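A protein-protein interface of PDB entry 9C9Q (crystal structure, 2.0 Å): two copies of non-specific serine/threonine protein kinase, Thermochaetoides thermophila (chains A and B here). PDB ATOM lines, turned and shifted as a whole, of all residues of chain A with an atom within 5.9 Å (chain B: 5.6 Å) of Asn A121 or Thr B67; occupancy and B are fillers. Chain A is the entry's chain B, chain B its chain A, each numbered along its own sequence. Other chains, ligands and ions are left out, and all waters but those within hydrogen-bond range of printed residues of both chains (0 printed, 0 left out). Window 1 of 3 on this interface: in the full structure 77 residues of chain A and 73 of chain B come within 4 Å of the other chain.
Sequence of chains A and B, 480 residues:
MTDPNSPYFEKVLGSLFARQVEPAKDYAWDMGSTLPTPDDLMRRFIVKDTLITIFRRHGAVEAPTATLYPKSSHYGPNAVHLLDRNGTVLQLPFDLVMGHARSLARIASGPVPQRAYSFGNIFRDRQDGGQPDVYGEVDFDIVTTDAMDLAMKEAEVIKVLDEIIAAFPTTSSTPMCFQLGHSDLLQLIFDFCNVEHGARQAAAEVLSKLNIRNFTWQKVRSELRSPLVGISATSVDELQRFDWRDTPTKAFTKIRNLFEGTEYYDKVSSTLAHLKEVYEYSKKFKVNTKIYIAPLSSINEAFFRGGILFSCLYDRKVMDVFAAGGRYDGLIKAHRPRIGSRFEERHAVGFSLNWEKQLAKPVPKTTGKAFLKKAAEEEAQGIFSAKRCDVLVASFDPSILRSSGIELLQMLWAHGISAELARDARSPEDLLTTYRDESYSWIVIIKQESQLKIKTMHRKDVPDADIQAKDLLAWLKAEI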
ATOM      1  N   THR A  65      16.440 -17.574  18.397  1.00  0.00           N
ATOM      2  CA  THR A  65      16.926 -18.708  17.629  1.00  0.00           C
ATOM      3  C   THR A  65      16.123 -18.889  16.347  1.00  0.00           C
ATOM      4  O   THR A  65      14.966 -18.476  16.239  1.00  0.00           O
ATOM      5  CB  THR A  65      16.882 -19.993  18.463  1.00  0.00           C
ATOM      6  OG1 THR A  65      15.567 -20.193  18.993  1.00  0.00           O
ATOM      7  CG2 THR A  65      17.845 -19.896  19.618  1.00  0.00           C
ATOM      8  N   THR A  67      13.953 -20.959  13.821  1.00  0.00           N
ATOM      9  CA  THR A  67      12.952 -22.001  14.027  1.00  0.00           C
ATOM     10  C   THR A  67      12.787 -22.925  12.837  1.00  0.00           C
ATOM     11  O   THR A  67      12.275 -24.039  12.995  1.00  0.00           O
ATOM     12  CB  THR A  67      11.586 -21.370  14.342  1.00  0.00           C
ATOM     13  OG1 THR A  67      11.773 -20.283  15.255  1.00  0.00           O
ATOM     14  CG2 THR A  67      10.664 -22.396  14.996  1.00  0.00           C
ATOM     15  N   LEU A  92      12.918 -28.544  11.107  1.00  0.00           N
ATOM     16  CA  LEU A  92      12.951 -27.953  12.424  1.00  0.00           C
ATOM     17  C   LEU A  92      14.330 -28.187  13.032  1.00  0.00           C
ATOM     18  O   LEU A  92      15.049 -29.102  12.628  1.00  0.00           O
ATOM     19  CB  LEU A  92      11.870 -28.566  13.306  1.00  0.00           C
ATOM     20  CG  LEU A  92      10.447 -28.370  12.779  1.00  0.00           C
ATOM     21  CD1 LEU A  92       9.474 -29.004  13.754  1.00  0.00           C
ATOM     22  CD2 LEU A  92      10.140 -26.889  12.573  1.00  0.00           C
ATOM     23  N   PRO A  93      14.731 -27.373  13.999  1.00  0.00           N
ATOM     24  CA  PRO A  93      16.077 -27.539  14.572  1.00  0.00           C
ATOM     25  C   PRO A  93      16.238 -28.914  15.205  1.00  0.00           C
ATOM     26  O   PRO A  93      15.376 -29.383  15.943  1.00  0.00           O
ATOM     27  CB  PRO A  93      16.160 -26.418  15.611  1.00  0.00           C
ATOM     28  CG  PRO A  93      15.146 -25.398  15.146  1.00  0.00           C
ATOM     29  CD  PRO A  93      14.019 -26.227  14.592  1.00  0.00           C
ATOM     30  N   ASP A  95      19.597 -29.487  16.489  1.00  0.00           N
ATOM     31  CA  ASP A  95      20.356 -28.846  17.550  1.00  0.00           C
ATOM     32  C   ASP A  95      20.187 -27.348  17.347  1.00  0.00           C
ATOM     33  O   ASP A  95      19.517 -26.910  16.405  1.00  0.00           O
ATOM     34  CB  ASP A  95      21.826 -29.271  17.490  1.00  0.00           C
ATOM     35  CG  ASP A  95      22.385 -29.112  16.104  1.00  0.00           C
ATOM     36  OD1 ASP A  95      22.442 -27.945  15.633  1.00  0.00           O
ATOM     37  OD2 ASP A  95      22.724 -30.143  15.468  1.00  0.00           O
ATOM     38  N   LEU A  96      20.793 -26.539  18.215  1.00  0.00           N
ATOM     39  CA  LEU A  96      20.663 -25.103  18.004  1.00  0.00           C
ATOM     40  C   LEU A  96      21.838 -24.496  17.238  1.00  0.00           C
ATOM     41  O   LEU A  96      21.725 -23.365  16.745  1.00  0.00           O
ATOM     42  CB  LEU A  96      20.498 -24.369  19.336  1.00  0.00           C
ATOM     43  CG  LEU A  96      19.244 -24.640  20.171  1.00  0.00           C
ATOM     44  CD1 LEU A  96      19.319 -23.809  21.448  1.00  0.00           C
ATOM     45  CD2 LEU A  96      17.912 -24.374  19.414  1.00  0.00           C
ATOM     46  N   PHE A 119      17.502 -20.088  24.606  1.00  0.00           N
ATOM     47  CA  PHE A 119      16.695 -21.241  24.988  1.00  0.00           C
ATOM     48  C   PHE A 119      15.793 -21.543  23.801  1.00  0.00           C
ATOM     49  O   PHE A 119      14.938 -20.728  23.445  1.00  0.00           O
ATOM     50  CB  PHE A 119      15.854 -20.960  26.234  1.00  0.00           C
ATOM     51  CG  PHE A 119      16.644 -20.804  27.502  1.00  0.00           C
ATOM     52  CD1 PHE A 119      17.181 -19.575  27.855  1.00  0.00           C
ATOM     53  CD2 PHE A 119      16.813 -21.875  28.365  1.00  0.00           C
ATOM     54  CE1 PHE A 119      17.898 -19.426  29.029  1.00  0.00           C
ATOM     55  CE2 PHE A 119      17.525 -21.726  29.547  1.00  0.00           C
ATOM     56  CZ  PHE A 119      18.062 -20.495  29.875  1.00  0.00           C
ATOM     57  N   GLY A 120      15.977 -22.703  23.184  1.00  0.00           N
ATOM     58  CA  GLY A 120      15.190 -23.077  22.027  1.00  0.00           C
ATOM     59  C   GLY A 120      14.737 -24.514  22.126  1.00  0.00           C
ATOM     60  O   GLY A 120      15.179 -25.282  22.993  1.00  0.00           O
ATOM     61  N   ASN A 121      13.822 -24.874  21.229  1.00  0.00           N
ATOM     62  CA  ASN A 121      13.330 -26.233  21.110  1.00  0.00           C
ATOM     63  C   ASN A 121      14.110 -26.958  20.027  1.00  0.00           C
ATOM     64  O   ASN A 121      14.446 -26.365  19.000  1.00  0.00           O
ATOM     65  CB  ASN A 121      11.844 -26.246  20.758  1.00  0.00           C
ATOM     66  CG  ASN A 121      11.002 -25.721  21.879  1.00  0.00           C
ATOM     67  OD1 ASN A 121      11.233 -26.057  23.038  1.00  0.00           O
ATOM     68  ND2 ASN A 121      10.019 -24.886  21.552  1.00  0.00           N
ATOM     69  N   ILE A 122      14.402 -28.238  20.273  1.00  0.00           N
ATOM     70  CA  ILE A 122      14.929 -29.144  19.265  1.00  0.00           C
ATOM     71  C   ILE A 122      13.966 -30.316  19.153  1.00  0.00           C
ATOM     72  O   ILE A 122      13.210 -30.615  20.082  1.00  0.00           O
ATOM     73  CB  ILE A 122      16.348 -29.634  19.581  1.00  0.00           C
ATOM     74  CG1 ILE A 122      16.376 -30.316  20.948  1.00  0.00           C
ATOM     75  CG2 ILE A 122      17.319 -28.469  19.548  1.00  0.00           C
ATOM     76  CD1 ILE A 122      17.702 -31.020  21.254  1.00  0.00           C
ATOM     77  N   PHE A 123      14.011 -30.995  18.008  1.00  0.00           N
ATOM     78  CA  PHE A 123      12.934 -31.901  17.643  1.00  0.00           C
ATOM     79  C   PHE A 123      13.466 -33.245  17.172  1.00  0.00           C
ATOM     80  O   PHE A 123      14.517 -33.332  16.534  1.00  0.00           O
ATOM     81  CB  PHE A 123      12.049 -31.269  16.558  1.00  0.00           C
ATOM     82  CG  PHE A 123      11.345 -30.039  17.025  1.00  0.00           C
ATOM     83  CD1 PHE A 123      11.966 -28.795  16.950  1.00  0.00           C
ATOM     84  CD2 PHE A 123      10.073 -30.128  17.558  1.00  0.00           C
ATOM     85  CE1 PHE A 123      11.323 -27.658  17.396  1.00  0.00           C
ATOM     86  CE2 PHE A 123       9.413 -28.992  18.011  1.00  0.00           C
ATOM     87  CZ  PHE A 123      10.038 -27.756  17.930  1.00  0.00           C
ATOM     88  N   VAL A 134       9.750 -33.179  21.506  1.00  0.00           N
ATOM     89  CA  VAL A 134      10.310 -31.843  21.673  1.00  0.00           C
ATOM     90  C   VAL A 134      11.152 -31.808  22.940  1.00  0.00           C
ATOM     91  O   VAL A 134      10.802 -32.432  23.946  1.00  0.00           O
ATOM     92  CB  VAL A 134       9.206 -30.769  21.727  1.00  0.00           C
ATOM     93  CG1 VAL A 134       9.814 -29.373  21.647  1.00  0.00           C
ATOM     94  CG2 VAL A 134       8.210 -30.989  20.593  1.00  0.00           C
ATOM     95  N   TYR A 135      12.247 -31.056  22.897  1.00  0.00           N
ATOM     96  CA  TYR A 135      13.200 -30.987  24.000  1.00  0.00           C
ATOM     97  C   TYR A 135      13.722 -29.565  24.134  1.00  0.00           C
ATOM     98  O   TYR A 135      13.899 -28.863  23.133  1.00  0.00           O
ATOM     99  CB  TYR A 135      14.382 -31.944  23.790  1.00  0.00           C
ATOM    100  CG  TYR A 135      13.981 -33.395  23.612  1.00  0.00           C
ATOM    101  CD1 TYR A 135      13.341 -34.095  24.634  1.00  0.00           C
ATOM    102  CD2 TYR A 135      14.247 -34.069  22.424  1.00  0.00           C
ATOM    103  CE1 TYR A 135      12.972 -35.425  24.470  1.00  0.00           C
ATOM    104  CE2 TYR A 135      13.881 -35.398  22.252  1.00  0.00           C
ATOM    105  CZ  TYR A 135      13.248 -36.070  23.277  1.00  0.00           C
ATOM    106  OH  TYR A 135      12.883 -37.388  23.099  1.00  0.00           O
ATOM    107  N   GLY A 136      13.964 -29.143  25.369  1.00  0.00           N
ATOM    108  CA  GLY A 136      14.545 -27.839  25.583  1.00  0.00           C
ATOM    109  C   GLY A 136      16.053 -27.909  25.569  1.00  0.00           C
ATOM    110  O   GLY A 136      16.645 -28.704  26.304  1.00  0.00           O
ATOM    111  N   GLU A 137      16.689 -27.099  24.730  1.00  0.00           N
ATOM    112  CA  GLU A 137      18.138 -26.971  24.714  1.00  0.00           C
ATOM    113  C   GLU A 137      18.502 -25.529  25.039  1.00  0.00           C
ATOM    114  O   GLU A 137      17.773 -24.592  24.696  1.00  0.00           O
ATOM    115  CB  GLU A 137      18.723 -27.409  23.337  1.00  0.00           C
ATOM    116  CG  GLU A 137      20.202 -27.091  23.125  1.00  0.00           C
ATOM    117  CD  GLU A 137      20.774 -27.687  21.813  1.00  0.00           C
ATOM    118  OE1 GLU A 137      20.440 -28.848  21.473  1.00  0.00           O
ATOM    119  OE2 GLU A 137      21.567 -26.999  21.120  1.00  0.00           O
ATOM    120  N   THR B  65       4.694 -24.262  24.948  1.00  0.00           N
ATOM    121  CA  THR B  65       3.782 -23.888  23.867  1.00  0.00           C
ATOM    122  C   THR B  65       3.910 -24.847  22.688  1.00  0.00           C
ATOM    123  O   THR B  65       5.016 -25.261  22.334  1.00  0.00           O
ATOM    124  CB  THR B  65       4.053 -22.455  23.374  1.00  0.00           C
ATOM    125  OG1 THR B  65       5.432 -22.311  23.023  1.00  0.00           O
ATOM    126  CG2 THR B  65       3.711 -21.434  24.441  1.00  0.00           C
ATOM    127  N   ALA B  66       2.779 -25.183  22.072  1.00  0.00           N
ATOM    128  CA  ALA B  66       2.808 -26.010  20.876  1.00  0.00           C
ATOM    129  C   ALA B  66       3.511 -25.267  19.748  1.00  0.00           C
ATOM    130  O   ALA B  66       3.254 -24.086  19.511  1.00  0.00           O
ATOM    131  CB  ALA B  66       1.385 -26.393  20.459  1.00  0.00           C
ATOM    132  N   THR B  67       4.405 -25.960  19.055  1.00  0.00           N
ATOM    133  CA  THR B  67       5.160 -25.372  17.953  1.00  0.00           C
ATOM    134  C   THR B  67       4.583 -25.694  16.584  1.00  0.00           C
ATOM    135  O   THR B  67       4.831 -24.951  15.633  1.00  0.00           O
ATOM    136  CB  THR B  67       6.612 -25.854  18.019  1.00  0.00           C
ATOM    137  OG1 THR B  67       7.133 -25.555  19.321  1.00  0.00           O
ATOM    138  CG2 THR B  67       7.476 -25.165  16.958  1.00  0.00           C
ATOM    139  N   LEU B  68       3.781 -26.750  16.476  1.00  0.00           N
ATOM    140  CA  LEU B  68       3.420 -27.314  15.187  1.00  0.00           C
ATOM    141  C   LEU B  68       2.148 -28.119  15.399  1.00  0.00           C
ATOM    142  O   LEU B  68       2.081 -28.895  16.353  1.00  0.00           O
ATOM    143  CB  LEU B  68       4.578 -28.201  14.692  1.00  0.00           C
ATOM    144  CG  LEU B  68       4.626 -28.859  13.324  1.00  0.00           C
ATOM    145  CD1 LEU B  68       4.862 -27.832  12.239  1.00  0.00           C
ATOM    146  CD2 LEU B  68       5.716 -29.900  13.315  1.00  0.00           C
ATOM    147  N   TYR B  69       1.148 -27.950  14.536  1.00  0.00           N
ATOM    148  CA  TYR B  69      -0.060 -28.754  14.673  1.00  0.00           C
ATOM    149  C   TYR B  69      -0.859 -28.685  13.374  1.00  0.00           C
ATOM    150  O   TYR B  69      -0.643 -27.785  12.550  1.00  0.00           O
ATOM    151  CB  TYR B  69      -0.907 -28.281  15.866  1.00  0.00           C
ATOM    152  CG  TYR B  69      -0.997 -26.790  16.014  1.00  0.00           C
ATOM    153  CD1 TYR B  69      -1.873 -26.052  15.235  1.00  0.00           C
ATOM    154  CD2 TYR B  69      -0.215 -26.116  16.956  1.00  0.00           C
ATOM    155  CE1 TYR B  69      -1.976 -24.671  15.380  1.00  0.00           C
ATOM    156  CE2 TYR B  69      -0.310 -24.740  17.112  1.00  0.00           C
ATOM    157  CZ  TYR B  69      -1.190 -24.022  16.312  1.00  0.00           C
ATOM    158  OH  TYR B  69      -1.285 -22.659  16.450  1.00  0.00           O
ATOM    159  N   GLN B  91       0.557 -26.293  10.456  1.00  0.00           N
ATOM    160  CA  GLN B  91       0.872 -24.878  10.489  1.00  0.00           C
ATOM    161  C   GLN B  91       1.796 -24.546  11.653  1.00  0.00           C
ATOM    162  O   GLN B  91       1.871 -25.265  12.653  1.00  0.00           O
ATOM    163  CB  GLN B  91      -0.385 -24.037  10.589  1.00  0.00           C
ATOM    164  CG  GLN B  91      -0.964 -24.020  11.960  1.00  0.00           C
ATOM    165  CD  GLN B  91      -2.034 -22.944  12.084  1.00  0.00           C
ATOM    166  OE1 GLN B  91      -3.211 -23.209  11.867  1.00  0.00           O
ATOM    167  NE2 GLN B  91      -1.619 -21.721  12.412  1.00  0.00           N
ATOM    168  N   LEU B  92       2.516 -23.455  11.489  1.00  0.00           N
ATOM    169  CA  LEU B  92       3.175 -22.782  12.588  1.00  0.00           C
ATOM    170  C   LEU B  92       2.174 -21.875  13.294  1.00  0.00           C
ATOM    171  O   LEU B  92       1.184 -21.444  12.686  1.00  0.00           O
ATOM    172  CB  LEU B  92       4.338 -21.959  12.071  1.00  0.00           C
ATOM    173  CG  LEU B  92       5.397 -22.699  11.242  1.00  0.00           C
ATOM    174  CD1 LEU B  92       6.560 -21.719  10.996  1.00  0.00           C
ATOM    175  CD2 LEU B  92       5.896 -23.915  11.979  1.00  0.00           C
ATOM    176  N   PRO B  93       2.401 -21.582  14.575  1.00  0.00           N
ATOM    177  CA  PRO B  93       1.460 -20.743  15.333  1.00  0.00           C
ATOM    178  C   PRO B  93       1.265 -19.385  14.677  1.00  0.00           C
ATOM    179  O   PRO B  93       2.222 -18.704  14.319  1.00  0.00           O
ATOM    180  CB  PRO B  93       2.143 -20.600  16.698  1.00  0.00           C
ATOM    181  CG  PRO B  93       3.010 -21.806  16.813  1.00  0.00           C
ATOM    182  CD  PRO B  93       3.517 -22.046  15.420  1.00  0.00           C
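Of the 15 printed residues of chain A, 3 touch a printed residue of chain B.
Hydrophobic or aromatic side chains of chain A that line the printed part of chain B: Leu A92 and Phe A123.
Hydrophobic or aromatic side chains of chain B within 4 Å of the printed part of chain A: Leu B68.
Among the printed residues, 3 pairs touch across the chains.
Among the printed residues, no Asp or Glu carboxylate lies within 4 Å of a Lys or Arg side-chain nitrogen of the other chain.
Of the printed residues of chain B, Leu A92 touches Leu B68 (3.9 Å).
Asp A95 touches none of the printed residues of chain B.
Of chain A, only Asn A121 (3.7 Å) and Phe A123 (3.8 Å) come within 4 Å of Thr B67.
Of the printed residues of chain A, Leu B68 touches Leu A92.
The nearest residue of chain A that does not touch Thr B67 is Thr A67 (4.7 Å).
4 positions are printed for both chains.
Leu B68 touches Leu A92 (CD2 to CD1, 3.9 Å).
OG1 of Thr B67 touches ND2 of Asn A121 (3.7 Å).
CZ of Phe A123 touches CG2 of Thr B67 (3.8 Å).
The backbone carbonyl oxygen (O) of Pro A93 sits at hydrogen-bond distance from the backbone NH (N) of Phe A123 (3.0 Å).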
